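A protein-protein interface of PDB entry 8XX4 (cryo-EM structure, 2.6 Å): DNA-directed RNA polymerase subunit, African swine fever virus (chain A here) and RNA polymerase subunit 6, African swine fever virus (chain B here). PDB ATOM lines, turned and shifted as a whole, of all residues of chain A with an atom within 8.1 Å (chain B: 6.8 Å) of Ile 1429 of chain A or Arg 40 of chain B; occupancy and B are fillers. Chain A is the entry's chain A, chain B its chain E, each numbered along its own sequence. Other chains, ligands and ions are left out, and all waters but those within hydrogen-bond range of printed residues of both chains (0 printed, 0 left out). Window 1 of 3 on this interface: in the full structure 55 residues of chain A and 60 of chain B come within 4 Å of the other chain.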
ATOM      1  N   TYR A   5     -14.192  -6.618  -4.497  1.00  0.00           N
ATOM      2  CA  TYR A   5     -15.566  -6.376  -4.087  1.00  0.00           C
ATOM      3  C   TYR A   5     -16.512  -6.603  -5.255  1.00  0.00           C
ATOM      4  O   TYR A   5     -16.305  -6.077  -6.350  1.00  0.00           O
ATOM      5  CB  TYR A   5     -15.710  -4.952  -3.560  1.00  0.00           C
ATOM      6  CG  TYR A   5     -17.117  -4.574  -3.170  1.00  0.00           C
ATOM      7  CD1 TYR A   5     -17.586  -4.805  -1.888  1.00  0.00           C
ATOM      8  CD2 TYR A   5     -17.975  -3.981  -4.082  1.00  0.00           C
ATOM      9  CE1 TYR A   5     -18.865  -4.456  -1.530  1.00  0.00           C
ATOM     10  CE2 TYR A   5     -19.252  -3.634  -3.731  1.00  0.00           C
ATOM     11  CZ  TYR A   5     -19.691  -3.870  -2.456  1.00  0.00           C
ATOM     12  OH  TYR A   5     -20.969  -3.521  -2.107  1.00  0.00           O
ATOM     13  N   GLU A   7     -20.913  -7.405  -6.320  1.00  0.00           N
ATOM     14  CA  GLU A   7     -22.318  -7.442  -5.957  1.00  0.00           C
ATOM     15  C   GLU A   7     -23.048  -8.340  -6.938  1.00  0.00           C
ATOM     16  O   GLU A   7     -22.707  -8.393  -8.119  1.00  0.00           O
ATOM     17  CB  GLU A   7     -22.940  -6.045  -5.963  1.00  0.00           C
ATOM     18  CG  GLU A   7     -22.815  -5.305  -4.651  1.00  0.00           C
ATOM     19  CD  GLU A   7     -23.210  -3.851  -4.769  1.00  0.00           C
ATOM     20  OE1 GLU A   7     -24.040  -3.532  -5.643  1.00  0.00           O
ATOM     21  OE2 GLU A   7     -22.686  -3.025  -3.994  1.00  0.00           O
ATOM     22  N   MET A 472     -21.600   4.986  10.328  1.00  0.00           N
ATOM     23  CA  MET A 472     -22.570   5.157   9.251  1.00  0.00           C
ATOM     24  C   MET A 472     -23.996   5.107   9.788  1.00  0.00           C
ATOM     25  O   MET A 472     -24.834   5.961   9.462  1.00  0.00           O
ATOM     26  CB  MET A 472     -22.356   4.070   8.202  1.00  0.00           C
ATOM     27  CG  MET A 472     -21.152   4.277   7.310  1.00  0.00           C
ATOM     28  SD  MET A 472     -21.426   3.655   5.648  1.00  0.00           S
ATOM     29  CE  MET A 472     -20.001   4.312   4.810  1.00  0.00           C
ATOM     30  N   VAL A 475     -24.702   8.248  11.850  1.00  0.00           N
ATOM     31  CA  VAL A 475     -24.937   9.395  10.979  1.00  0.00           C
ATOM     32  C   VAL A 475     -26.354   9.356  10.442  1.00  0.00           C
ATOM     33  O   VAL A 475     -27.085  10.352  10.478  1.00  0.00           O
ATOM     34  CB  VAL A 475     -23.918   9.415   9.827  1.00  0.00           C
ATOM     35  CG1 VAL A 475     -24.476  10.201   8.660  1.00  0.00           C
ATOM     36  CG2 VAL A 475     -22.610   9.998  10.276  1.00  0.00           C
ATOM     37  N   GLU A 476     -26.767   8.198   9.948  1.00  0.00           N
ATOM     38  CA  GLU A 476     -28.070   8.110   9.312  1.00  0.00           C
ATOM     39  C   GLU A 476     -29.213   8.107  10.319  1.00  0.00           C
ATOM     40  O   GLU A 476     -30.300   8.608  10.016  1.00  0.00           O
ATOM     41  CB  GLU A 476     -28.101   6.877   8.431  1.00  0.00           C
ATOM     42  CG  GLU A 476     -29.434   6.294   8.232  1.00  0.00           C
ATOM     43  CD  GLU A 476     -29.301   4.864   7.895  1.00  0.00           C
ATOM     44  OE1 GLU A 476     -28.651   4.591   6.875  1.00  0.00           O
ATOM     45  OE2 GLU A 476     -29.809   4.024   8.657  1.00  0.00           O
ATOM     46  N   LEU A 479     -29.502  11.873  10.970  1.00  0.00           N
ATOM     47  CA  LEU A 479     -29.904  12.714   9.848  1.00  0.00           C
ATOM     48  C   LEU A 479     -31.174  12.247   9.156  1.00  0.00           C
ATOM     49  O   LEU A 479     -31.841  13.054   8.502  1.00  0.00           O
ATOM     50  CB  LEU A 479     -28.783  12.780   8.811  1.00  0.00           C
ATOM     51  CG  LEU A 479     -27.510  13.525   9.189  1.00  0.00           C
ATOM     52  CD1 LEU A 479     -26.672  13.774   7.954  1.00  0.00           C
ATOM     53  CD2 LEU A 479     -27.850  14.821   9.882  1.00  0.00           C
ATOM     54  N   LEU A 480     -31.523  10.978   9.264  1.00  0.00           N
ATOM     55  CA  LEU A 480     -32.604  10.434   8.456  1.00  0.00           C
ATOM     56  C   LEU A 480     -33.754   9.868   9.265  1.00  0.00           C
ATOM     57  O   LEU A 480     -34.911  10.069   8.899  1.00  0.00           O
ATOM     58  CB  LEU A 480     -32.056   9.348   7.529  1.00  0.00           C
ATOM     59  CG  LEU A 480     -32.968   8.875   6.408  1.00  0.00           C
ATOM     60  CD1 LEU A 480     -32.919   9.851   5.258  1.00  0.00           C
ATOM     61  CD2 LEU A 480     -32.544   7.495   5.968  1.00  0.00           C
ATOM     62  N   ILE A1422     -31.827   1.004  -2.283  1.00  0.00           N
ATOM     63  CA  ILE A1422     -32.826   2.047  -2.103  1.00  0.00           C
ATOM     64  C   ILE A1422     -32.373   2.943  -0.961  1.00  0.00           C
ATOM     65  O   ILE A1422     -31.426   2.635  -0.239  1.00  0.00           O
ATOM     66  CB  ILE A1422     -34.232   1.497  -1.793  1.00  0.00           C
ATOM     67  CG1 ILE A1422     -34.305   1.081  -0.331  1.00  0.00           C
ATOM     68  CG2 ILE A1422     -34.598   0.336  -2.697  1.00  0.00           C
ATOM     69  CD1 ILE A1422     -35.669   1.113   0.206  1.00  0.00           C
ATOM     70  N   GLY A1423     -33.077   4.053  -0.792  1.00  0.00           N
ATOM     71  CA  GLY A1423     -32.816   4.913   0.347  1.00  0.00           C
ATOM     72  C   GLY A1423     -31.450   5.547   0.254  1.00  0.00           C
ATOM     73  O   GLY A1423     -31.061   6.079  -0.788  1.00  0.00           O
ATOM     74  N   THR A1424     -30.700   5.491   1.356  1.00  0.00           N
ATOM     75  CA  THR A1424     -29.379   6.106   1.389  1.00  0.00           C
ATOM     76  C   THR A1424     -28.414   5.451   0.417  1.00  0.00           C
ATOM     77  O   THR A1424     -27.379   6.039   0.096  1.00  0.00           O
ATOM     78  CB  THR A1424     -28.796   6.052   2.801  1.00  0.00           C
ATOM     79  OG1 THR A1424     -28.945   4.733   3.331  1.00  0.00           O
ATOM     80  CG2 THR A1424     -29.504   7.034   3.705  1.00  0.00           C
ATOM     81  N   MET A1425     -28.730   4.256  -0.069  1.00  0.00           N
ATOM     82  CA  MET A1425     -27.857   3.532  -0.979  1.00  0.00           C
ATOM     83  C   MET A1425     -28.428   3.433  -2.386  1.00  0.00           C
ATOM     84  O   MET A1425     -28.023   2.561  -3.155  1.00  0.00           O
ATOM     85  CB  MET A1425     -27.563   2.152  -0.404  1.00  0.00           C
ATOM     86  CG  MET A1425     -26.710   2.217   0.851  1.00  0.00           C
ATOM     87  SD  MET A1425     -26.541   0.620   1.630  1.00  0.00           S
ATOM     88  CE  MET A1425     -27.695  -0.299   0.630  1.00  0.00           C
ATOM     89  N   TYR A1426     -29.362   4.316  -2.737  1.00  0.00           N
ATOM     90  CA  TYR A1426     -29.848   4.365  -4.109  1.00  0.00           C
ATOM     91  C   TYR A1426     -28.792   4.933  -5.045  1.00  0.00           C
ATOM     92  O   TYR A1426     -28.533   4.370  -6.114  1.00  0.00           O
ATOM     93  CB  TYR A1426     -31.127   5.194  -4.183  1.00  0.00           C
ATOM     94  CG  TYR A1426     -31.860   5.033  -5.485  1.00  0.00           C
ATOM     95  CD1 TYR A1426     -32.417   3.819  -5.835  1.00  0.00           C
ATOM     96  CD2 TYR A1426     -31.995   6.093  -6.365  1.00  0.00           C
ATOM     97  CE1 TYR A1426     -33.083   3.662  -7.019  1.00  0.00           C
ATOM     98  CE2 TYR A1426     -32.662   5.944  -7.554  1.00  0.00           C
ATOM     99  CZ  TYR A1426     -33.203   4.725  -7.875  1.00  0.00           C
ATOM    100  OH  TYR A1426     -33.870   4.552  -9.058  1.00  0.00           O
ATOM    101  N   SER A1427     -28.174   6.043  -4.663  1.00  0.00           N
ATOM    102  CA  SER A1427     -27.096   6.651  -5.425  1.00  0.00           C
ATOM    103  C   SER A1427     -25.773   6.194  -4.843  1.00  0.00           C
ATOM    104  O   SER A1427     -25.609   6.161  -3.619  1.00  0.00           O
ATOM    105  CB  SER A1427     -27.184   8.176  -5.393  1.00  0.00           C
ATOM    106  OG  SER A1427     -28.395   8.633  -5.961  1.00  0.00           O
ATOM    107  N   ASP A1428     -24.839   5.829  -5.708  1.00  0.00           N
ATOM    108  CA  ASP A1428     -23.547   5.372  -5.237  1.00  0.00           C
ATOM    109  C   ASP A1428     -22.557   6.523  -5.205  1.00  0.00           C
ATOM    110  O   ASP A1428     -22.571   7.410  -6.059  1.00  0.00           O
ATOM    111  CB  ASP A1428     -23.016   4.235  -6.104  1.00  0.00           C
ATOM    112  CG  ASP A1428     -23.264   4.457  -7.565  1.00  0.00           C
ATOM    113  OD1 ASP A1428     -24.443   4.579  -7.958  1.00  0.00           O
ATOM    114  OD2 ASP A1428     -22.277   4.486  -8.324  1.00  0.00           O
ATOM    115  N   ILE A1429     -21.701   6.500  -4.193  1.00  0.00           N
ATOM    116  CA  ILE A1429     -20.729   7.553  -3.946  1.00  0.00           C
ATOM    117  C   ILE A1429     -19.401   7.135  -4.549  1.00  0.00           C
ATOM    118  O   ILE A1429     -18.956   5.999  -4.364  1.00  0.00           O
ATOM    119  CB  ILE A1429     -20.586   7.832  -2.442  1.00  0.00           C
ATOM    120  CG1 ILE A1429     -21.960   8.012  -1.808  1.00  0.00           C
ATOM    121  CG2 ILE A1429     -19.725   9.046  -2.206  1.00  0.00           C
ATOM    122  CD1 ILE A1429     -22.789   9.097  -2.444  1.00  0.00           C
ATOM    123  N   ILE A1430     -18.780   8.046  -5.284  1.00  0.00           N
ATOM    124  CA  ILE A1430     -17.430   7.857  -5.779  1.00  0.00           C
ATOM    125  C   ILE A1430     -16.560   8.948  -5.176  1.00  0.00           C
ATOM    126  O   ILE A1430     -17.040  10.004  -4.761  1.00  0.00           O
ATOM    127  CB  ILE A1430     -17.368   7.874  -7.318  1.00  0.00           C
ATOM    128  CG1 ILE A1430     -17.454   9.300  -7.843  1.00  0.00           C
ATOM    129  CG2 ILE A1430     -18.496   7.056  -7.897  1.00  0.00           C
ATOM    130  CD1 ILE A1430     -17.463   9.393  -9.340  1.00  0.00           C
ATOM    131  N   MET A1431     -15.264   8.678  -5.111  1.00  0.00           N
ATOM    132  CA  MET A1431     -14.313   9.591  -4.494  1.00  0.00           C
ATOM    133  C   MET A1431     -13.913  10.659  -5.499  1.00  0.00           C
ATOM    134  O   MET A1431     -13.695  10.358  -6.677  1.00  0.00           O
ATOM    135  CB  MET A1431     -13.079   8.840  -3.995  1.00  0.00           C
ATOM    136  CG  MET A1431     -13.386   7.675  -3.079  1.00  0.00           C
ATOM    137  SD  MET A1431     -13.596   8.090  -1.339  1.00  0.00           S
ATOM    138  CE  MET A1431     -12.600   9.553  -1.179  1.00  0.00           C
ATOM    139  N   ASP A1432     -13.831  11.905  -5.037  1.00  0.00           N
ATOM    140  CA  ASP A1432     -13.447  13.018  -5.895  1.00  0.00           C
ATOM    141  C   ASP A1432     -11.937  13.059  -6.074  1.00  0.00           C
ATOM    142  O   ASP A1432     -11.233  13.711  -5.301  1.00  0.00           O
ATOM    143  CB  ASP A1432     -13.948  14.336  -5.313  1.00  0.00           C
ATOM    144  CG  ASP A1432     -14.209  15.375  -6.371  1.00  0.00           C
ATOM    145  OD1 ASP A1432     -13.697  15.226  -7.498  1.00  0.00           O
ATOM    146  OD2 ASP A1432     -14.932  16.346  -6.076  1.00  0.00           O
ATOM    147  N   THR B  34     -30.732  14.855  -2.412  1.00  0.00           N
ATOM    148  CA  THR B  34     -31.807  14.270  -1.633  1.00  0.00           C
ATOM    149  C   THR B  34     -31.331  14.036  -0.206  1.00  0.00           C
ATOM    150  O   THR B  34     -30.134  14.025   0.080  1.00  0.00           O
ATOM    151  CB  THR B  34     -32.289  12.960  -2.257  1.00  0.00           C
ATOM    152  OG1 THR B  34     -31.244  11.988  -2.213  1.00  0.00           O
ATOM    153  CG2 THR B  34     -32.698  13.178  -3.697  1.00  0.00           C
ATOM    154  N   THR B  35     -32.289  13.874   0.704  1.00  0.00           N
ATOM    155  CA  THR B  35     -31.930  13.571   2.083  1.00  0.00           C
ATOM    156  C   THR B  35     -31.174  12.254   2.168  1.00  0.00           C
ATOM    157  O   THR B  35     -30.237  12.118   2.961  1.00  0.00           O
ATOM    158  CB  THR B  35     -33.182  13.535   2.957  1.00  0.00           C
ATOM    159  OG1 THR B  35     -34.005  14.666   2.657  1.00  0.00           O
ATOM    160  CG2 THR B  35     -32.807  13.577   4.423  1.00  0.00           C
ATOM    161  N   PHE B  36     -31.559  11.277   1.345  1.00  0.00           N
ATOM    162  CA  PHE B  36     -30.815  10.025   1.265  1.00  0.00           C
ATOM    163  C   PHE B  36     -29.387  10.266   0.805  1.00  0.00           C
ATOM    164  O   PHE B  36     -28.438   9.727   1.379  1.00  0.00           O
ATOM    165  CB  PHE B  36     -31.511   9.063   0.308  1.00  0.00           C
ATOM    166  CG  PHE B  36     -32.870   8.638   0.753  1.00  0.00           C
ATOM    167  CD1 PHE B  36     -33.136   8.403   2.085  1.00  0.00           C
ATOM    168  CD2 PHE B  36     -33.880   8.453  -0.169  1.00  0.00           C
ATOM    169  CE1 PHE B  36     -34.384   8.007   2.487  1.00  0.00           C
ATOM    170  CE2 PHE B  36     -35.126   8.055   0.231  1.00  0.00           C
ATOM    171  CZ  PHE B  36     -35.380   7.833   1.558  1.00  0.00           C
ATOM    172  N   GLU B  37     -29.218  11.070  -0.244  1.00  0.00           N
ATOM    173  CA  GLU B  37     -27.890  11.304  -0.795  1.00  0.00           C
ATOM    174  C   GLU B  37     -27.011  12.073   0.179  1.00  0.00           C
ATOM    175  O   GLU B  37     -25.839  11.735   0.358  1.00  0.00           O
ATOM    176  CB  GLU B  37     -27.996  12.054  -2.118  1.00  0.00           C
ATOM    177  CG  GLU B  37     -28.170  11.159  -3.319  1.00  0.00           C
ATOM    178  CD  GLU B  37     -28.805  11.874  -4.488  1.00  0.00           C
ATOM    179  OE1 GLU B  37     -28.883  13.118  -4.458  1.00  0.00           O
ATOM    180  OE2 GLU B  37     -29.236  11.188  -5.434  1.00  0.00           O
ATOM    181  N   ALA B  38     -27.552  13.117   0.806  1.00  0.00           N
ATOM    182  CA  ALA B  38     -26.772  13.874   1.778  1.00  0.00           C
ATOM    183  C   ALA B  38     -26.414  13.017   2.982  1.00  0.00           C
ATOM    184  O   ALA B  38     -25.290  13.085   3.494  1.00  0.00           O
ATOM    185  CB  ALA B  38     -27.543  15.117   2.208  1.00  0.00           C
ATOM    186  N   THR B  39     -27.359  12.197   3.445  1.00  0.00           N
ATOM    187  CA  THR B  39     -27.085  11.301   4.559  1.00  0.00           C
ATOM    188  C   THR B  39     -25.993  10.300   4.207  1.00  0.00           C
ATOM    189  O   THR B  39     -25.096  10.043   5.014  1.00  0.00           O
ATOM    190  CB  THR B  39     -28.365  10.576   4.963  1.00  0.00           C
ATOM    191  OG1 THR B  39     -29.358  11.538   5.330  1.00  0.00           O
ATOM    192  CG2 THR B  39     -28.111   9.664   6.129  1.00  0.00           C
ATOM    193  N   ARG B  40     -26.050   9.727   3.004  1.00  0.00           N
ATOM    194  CA  ARG B  40     -25.025   8.781   2.584  1.00  0.00           C
ATOM    195  C   ARG B  40     -23.671   9.457   2.437  1.00  0.00           C
ATOM    196  O   ARG B  40     -22.643   8.873   2.786  1.00  0.00           O
ATOM    197  CB  ARG B  40     -25.427   8.121   1.273  1.00  0.00           C
ATOM    198  CG  ARG B  40     -24.345   7.273   0.656  1.00  0.00           C
ATOM    199  CD  ARG B  40     -24.299   5.901   1.277  1.00  0.00           C
ATOM    200  NE  ARG B  40     -23.419   5.003   0.539  1.00  0.00           N
ATOM    201  CZ  ARG B  40     -22.750   4.000   1.085  1.00  0.00           C
ATOM    202  NH1 ARG B  40     -22.841   3.733   2.375  1.00  0.00           N
ATOM    203  NH2 ARG B  40     -21.969   3.249   0.318  1.00  0.00           N
ATOM    204  N   LEU B  41     -23.646  10.680   1.908  1.00  0.00           N
ATOM    205  CA  LEU B  41     -22.390  11.406   1.791  1.00  0.00           C
ATOM    206  C   LEU B  41     -21.769  11.637   3.157  1.00  0.00           C
ATOM    207  O   LEU B  41     -20.571  11.407   3.355  1.00  0.00           O
ATOM    208  CB  LEU B  41     -22.618  12.740   1.086  1.00  0.00           C
ATOM    209  CG  LEU B  41     -22.804  12.710  -0.424  1.00  0.00           C
ATOM    210  CD1 LEU B  41     -23.527  13.959  -0.839  1.00  0.00           C
ATOM    211  CD2 LEU B  41     -21.472  12.606  -1.122  1.00  0.00           C
ATOM    212  N   VAL B  42     -22.574  12.082   4.120  1.00  0.00           N
ATOM    213  CA  VAL B  42     -22.042  12.343   5.451  1.00  0.00           C
ATOM    214  C   VAL B  42     -21.599  11.047   6.115  1.00  0.00           C
ATOM    215  O   VAL B  42     -20.574  11.009   6.798  1.00  0.00           O
ATOM    216  CB  VAL B  42     -23.075  13.103   6.302  1.00  0.00           C
ATOM    217  CG1 VAL B  42     -22.610  13.207   7.738  1.00  0.00           C
ATOM    218  CG2 VAL B  42     -23.292  14.476   5.732  1.00  0.00           C
ATOM    219  N   ALA B  43     -22.346   9.961   5.910  1.00  0.00           N
ATOM    220  CA  ALA B  43     -21.978   8.684   6.513  1.00  0.00           C
ATOM    221  C   ALA B  43     -20.672   8.153   5.939  1.00  0.00           C
ATOM    222  O   ALA B  43     -19.795   7.694   6.680  1.00  0.00           O
ATOM    223  CB  ALA B  43     -23.103   7.671   6.315  1.00  0.00           C
ATOM    224  N   VAL B  44     -20.524   8.205   4.614  1.00  0.00           N
ATOM    225  CA  VAL B  44     -19.296   7.745   3.977  1.00  0.00           C
ATOM    226  C   VAL B  44     -18.119   8.598   4.420  1.00  0.00           C
ATOM    227  O   VAL B  44     -17.051   8.079   4.762  1.00  0.00           O
ATOM    228  CB  VAL B  44     -19.456   7.752   2.446  1.00  0.00           C
ATOM    229  CG1 VAL B  44     -18.113   7.602   1.771  1.00  0.00           C
ATOM    230  CG2 VAL B  44     -20.386   6.652   2.011  1.00  0.00           C
ATOM    231  N   ARG B  45     -18.300   9.920   4.435  1.00  0.00           N
ATOM    232  CA  ARG B  45     -17.225  10.808   4.852  1.00  0.00           C
ATOM    233  C   ARG B  45     -16.842  10.572   6.305  1.00  0.00           C
ATOM    234  O   ARG B  45     -15.659  10.582   6.648  1.00  0.00           O
ATOM    235  CB  ARG B  45     -17.639  12.259   4.632  1.00  0.00           C
ATOM    236  CG  ARG B  45     -16.530  13.259   4.842  1.00  0.00           C
ATOM    237  CD  ARG B  45     -15.258  12.827   4.153  1.00  0.00           C
ATOM    238  NE  ARG B  45     -14.162  13.745   4.432  1.00  0.00           N
ATOM    239  CZ  ARG B  45     -12.884  13.401   4.445  1.00  0.00           C
ATOM    240  NH1 ARG B  45     -12.501  12.160   4.203  1.00  0.00           N
ATOM    241  NH2 ARG B  45     -11.968  14.326   4.706  1.00  0.00           N
ATOM    242  N   ALA B  46     -17.826  10.354   7.175  1.00  0.00           N
ATOM    243  CA  ALA B  46     -17.531  10.147   8.585  1.00  0.00           C
ATOM    244  C   ALA B  46     -16.831   8.815   8.819  1.00  0.00           C
ATOM    245  O   ALA B  46     -15.903   8.733   9.628  1.00  0.00           O
ATOM    246  CB  ALA B  46     -18.815  10.243   9.400  1.00  0.00           C
ATOM    247  N   GLN B  48     -14.913   7.329   6.627  1.00  0.00           N
ATOM    248  CA  GLN B  48     -13.564   7.514   6.108  1.00  0.00           C
ATOM    249  C   GLN B  48     -12.714   8.357   7.049  1.00  0.00           C
ATOM    250  O   GLN B  48     -11.508   8.128   7.172  1.00  0.00           O
ATOM    251  CB  GLN B  48     -13.626   8.135   4.720  1.00  0.00           C
ATOM    252  CG  GLN B  48     -14.051   7.148   3.665  1.00  0.00           C
ATOM    253  CD  GLN B  48     -14.289   7.797   2.336  1.00  0.00           C
ATOM    254  OE1 GLN B  48     -14.229   9.017   2.211  1.00  0.00           O
ATOM    255  NE2 GLN B  48     -14.557   6.989   1.326  1.00  0.00           N
ATOM    256  N   LEU B  79     -16.183  13.858  -1.774  1.00  0.00           N
ATOM    257  CA  LEU B  79     -16.925  12.806  -2.447  1.00  0.00           C
ATOM    258  C   LEU B  79     -17.715  13.362  -3.621  1.00  0.00           C
ATOM    259  O   LEU B  79     -17.943  14.566  -3.735  1.00  0.00           O
ATOM    260  CB  LEU B  79     -17.871  12.102  -1.472  1.00  0.00           C
ATOM    261  CG  LEU B  79     -17.233  11.599  -0.183  1.00  0.00           C
ATOM    262  CD1 LEU B  79     -18.287  11.384   0.873  1.00  0.00           C
ATOM    263  CD2 LEU B  79     -16.478  10.322  -0.454  1.00  0.00           C
ATOM    264  N   LEU B  80     -18.125  12.457  -4.503  1.00  0.00           N
ATOM    265  CA  LEU B  80     -19.003  12.773  -5.615  1.00  0.00           C
ATOM    266  C   LEU B  80     -20.197  11.832  -5.583  1.00  0.00           C
ATOM    267  O   LEU B  80     -20.114  10.708  -5.088  1.00  0.00           O
ATOM    268  CB  LEU B  80     -18.290  12.649  -6.966  1.00  0.00           C
ATOM    269  CG  LEU B  80     -17.224  13.668  -7.358  1.00  0.00           C
ATOM    270  CD1 LEU B  80     -16.568  13.237  -8.642  1.00  0.00           C
ATOM    271  CD2 LEU B  80     -17.818  15.048  -7.510  1.00  0.00           C
ATOM    272  N   VAL B  81     -21.315  12.304  -6.123  1.00  0.00           N
ATOM    273  CA  VAL B  81     -22.543  11.524  -6.218  1.00  0.00           C
ATOM    274  C   VAL B  81     -22.716  11.106  -7.666  1.00  0.00           C
ATOM    275  O   VAL B  81     -22.725  11.954  -8.565  1.00  0.00           O
ATOM    276  CB  VAL B  81     -23.761  12.323  -5.731  1.00  0.00           C
ATOM    277  CG1 VAL B  81     -25.008  11.476  -5.813  1.00  0.00           C
ATOM    278  CG2 VAL B  81     -23.542  12.808  -4.321  1.00  0.00           C
ATOM    279  N   MET B  82     -22.850   9.808  -7.899  1.00  0.00           N
ATOM    280  CA  MET B  82     -23.057   9.286  -9.241  1.00  0.00           C
ATOM    281  C   MET B  82     -24.442   8.660  -9.314  1.00  0.00           C
ATOM    282  O   MET B  82     -24.749   7.734  -8.559  1.00  0.00           O
ATOM    283  CB  MET B  82     -21.978   8.275  -9.619  1.00  0.00           C
ATOM    284  CG  MET B  82     -22.334   7.438 -10.823  1.00  0.00           C
ATOM    285  SD  MET B  82     -21.479   5.864 -10.879  1.00  0.00           S
ATOM    286  CE  MET B  82     -19.952   6.383 -11.639  1.00  0.00           C
ATOM    287  N   PRO B 100     -21.284  17.326  -4.891  1.00  0.00           N
ATOM    288  CA  PRO B 100     -22.008  17.798  -3.700  1.00  0.00           C
ATOM    289  C   PRO B 100     -21.575  19.168  -3.226  1.00  0.00           C
ATOM    290  O   PRO B 100     -22.361  19.854  -2.567  1.00  0.00           O
ATOM    291  CB  PRO B 100     -21.696  16.726  -2.649  1.00  0.00           C
ATOM    292  CG  PRO B 100     -21.246  15.553  -3.411  1.00  0.00           C
ATOM    293  CD  PRO B 100     -20.573  16.067  -4.634  1.00  0.00           C
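The backbone NH (N) of Glu 37 of chain B lies within hydrogen-bond range of the side-chain hydroxyl (OG1) of Thr 34 of chain B (3.0 Å).
The backbone carbonyl oxygen of Thr 35 of chain B is in hydrogen-bond range of the side-chain hydroxyl of Thr 39 of chain B, at 2.6 Å.
Printed residues of chain B that touch a printed residue of chain A: Thr 35, Phe 36, Glu 37, Thr 39, Arg 40, Leu 41, Val 42, Ala 43, Val 44, Ala 46, Gln 48, Leu 79, Leu 80, Val 81 and Met 82.
Hydrophobic or aromatic side chains of chain B within 4 Å of the printed part of chain A: Phe 36, Leu 41, Val 42, Ala 43, Val 44, Ala 46, Leu 79, Leu 80, Val 81 and Met 82.
Among the printed residues, 28 pairs touch across the chains.
Met 472 of chain A touches Val 44 of chain B (CE to CA, 3.6 Å).
O of Thr 39 of chain B touches CG1 of Val 475 of chain A, 3.7 Å away.
Val 475 of chain A touches Val 42 of chain B (CG1 to CG1, 3.7 Å).
Thr 39 of chain B touches Glu 476 of chain A.
OG1 of Thr 39 of chain B touches CB of Leu 479 of chain A, 3.7 Å away.
Thr 39 of chain B touches Leu 480 of chain A (OG1 to CD1, 3.9 Å).
Ser 1427 of chain A touches Val 81 of chain B.
Ile 1430 of chain A touches Leu 79 of chain B (O to C, 3.6 Å).
SD of Met 1431 of chain A touches CD2 of Leu 79 of chain B, at 3.8 Å.
CD2 of Leu 80 of chain B touches OD2 of Asp 1432 of chain A, at 3.5 Å.
Of chain B, only Arg 40, Leu 41, Leu 79 and Leu 80 come within 4 Å of Ile 1429 of chain A.
Of the printed residues of chain A, Met 82 of chain B touches Asp 1428 (3.0 Å).
Printed residues of chain A within 4 Å of Leu 79 of chain B: Ile 1429 (3.6 Å), Ile 1430 (3.6 Å) and Met 1431 (3.8 Å).
Printed residues of chain A within 4 Å of Gln 48 of chain B: Met 1431.
Of the printed residues of chain A, Ala 43 of chain B touches Met 472 and Val 475.
Of the printed residues of chain B, Leu 479 of chain A touches Thr 39.
Thr 34 of chain B touches none of the printed residues of chain A.
Ala 38 of chain B touches none of the printed residues of chain A.
The nearest residue of chain A that does not touch Arg 40 of chain B is Met 1425 of chain A (4.3 Å).
The nearest printed residue of chain B that does not touch Ile 1430 of chain A is Met 82 of chain B (4.1 Å).
SD of Met 472 of chain A sits at hydrogen-bond distance from NH1 of Arg 40 of chain B, at 3.6 Å.
The side-chain hydroxyl (OG) of Ser 1427 of chain A lies within hydrogen-bond range of the side-chain carboxylate (OE2) of Glu 37 of chain B.
O of Asp 1428 of chain A lies within hydrogen-bond range of N of Met 82 of chain B (3.0 Å).
The backbone carbonyl oxygen of Ile 1430 of chain A sits at hydrogen-bond distance from the backbone NH of Leu 80 of chain B, 2.7 Å away.
The side-chain amide nitrogen (NE2) of Gln 48 of chain B is in hydrogen-bond range of the side-chain sulfur (SD) of Met 1431 of chain A, at 3.0 Å.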
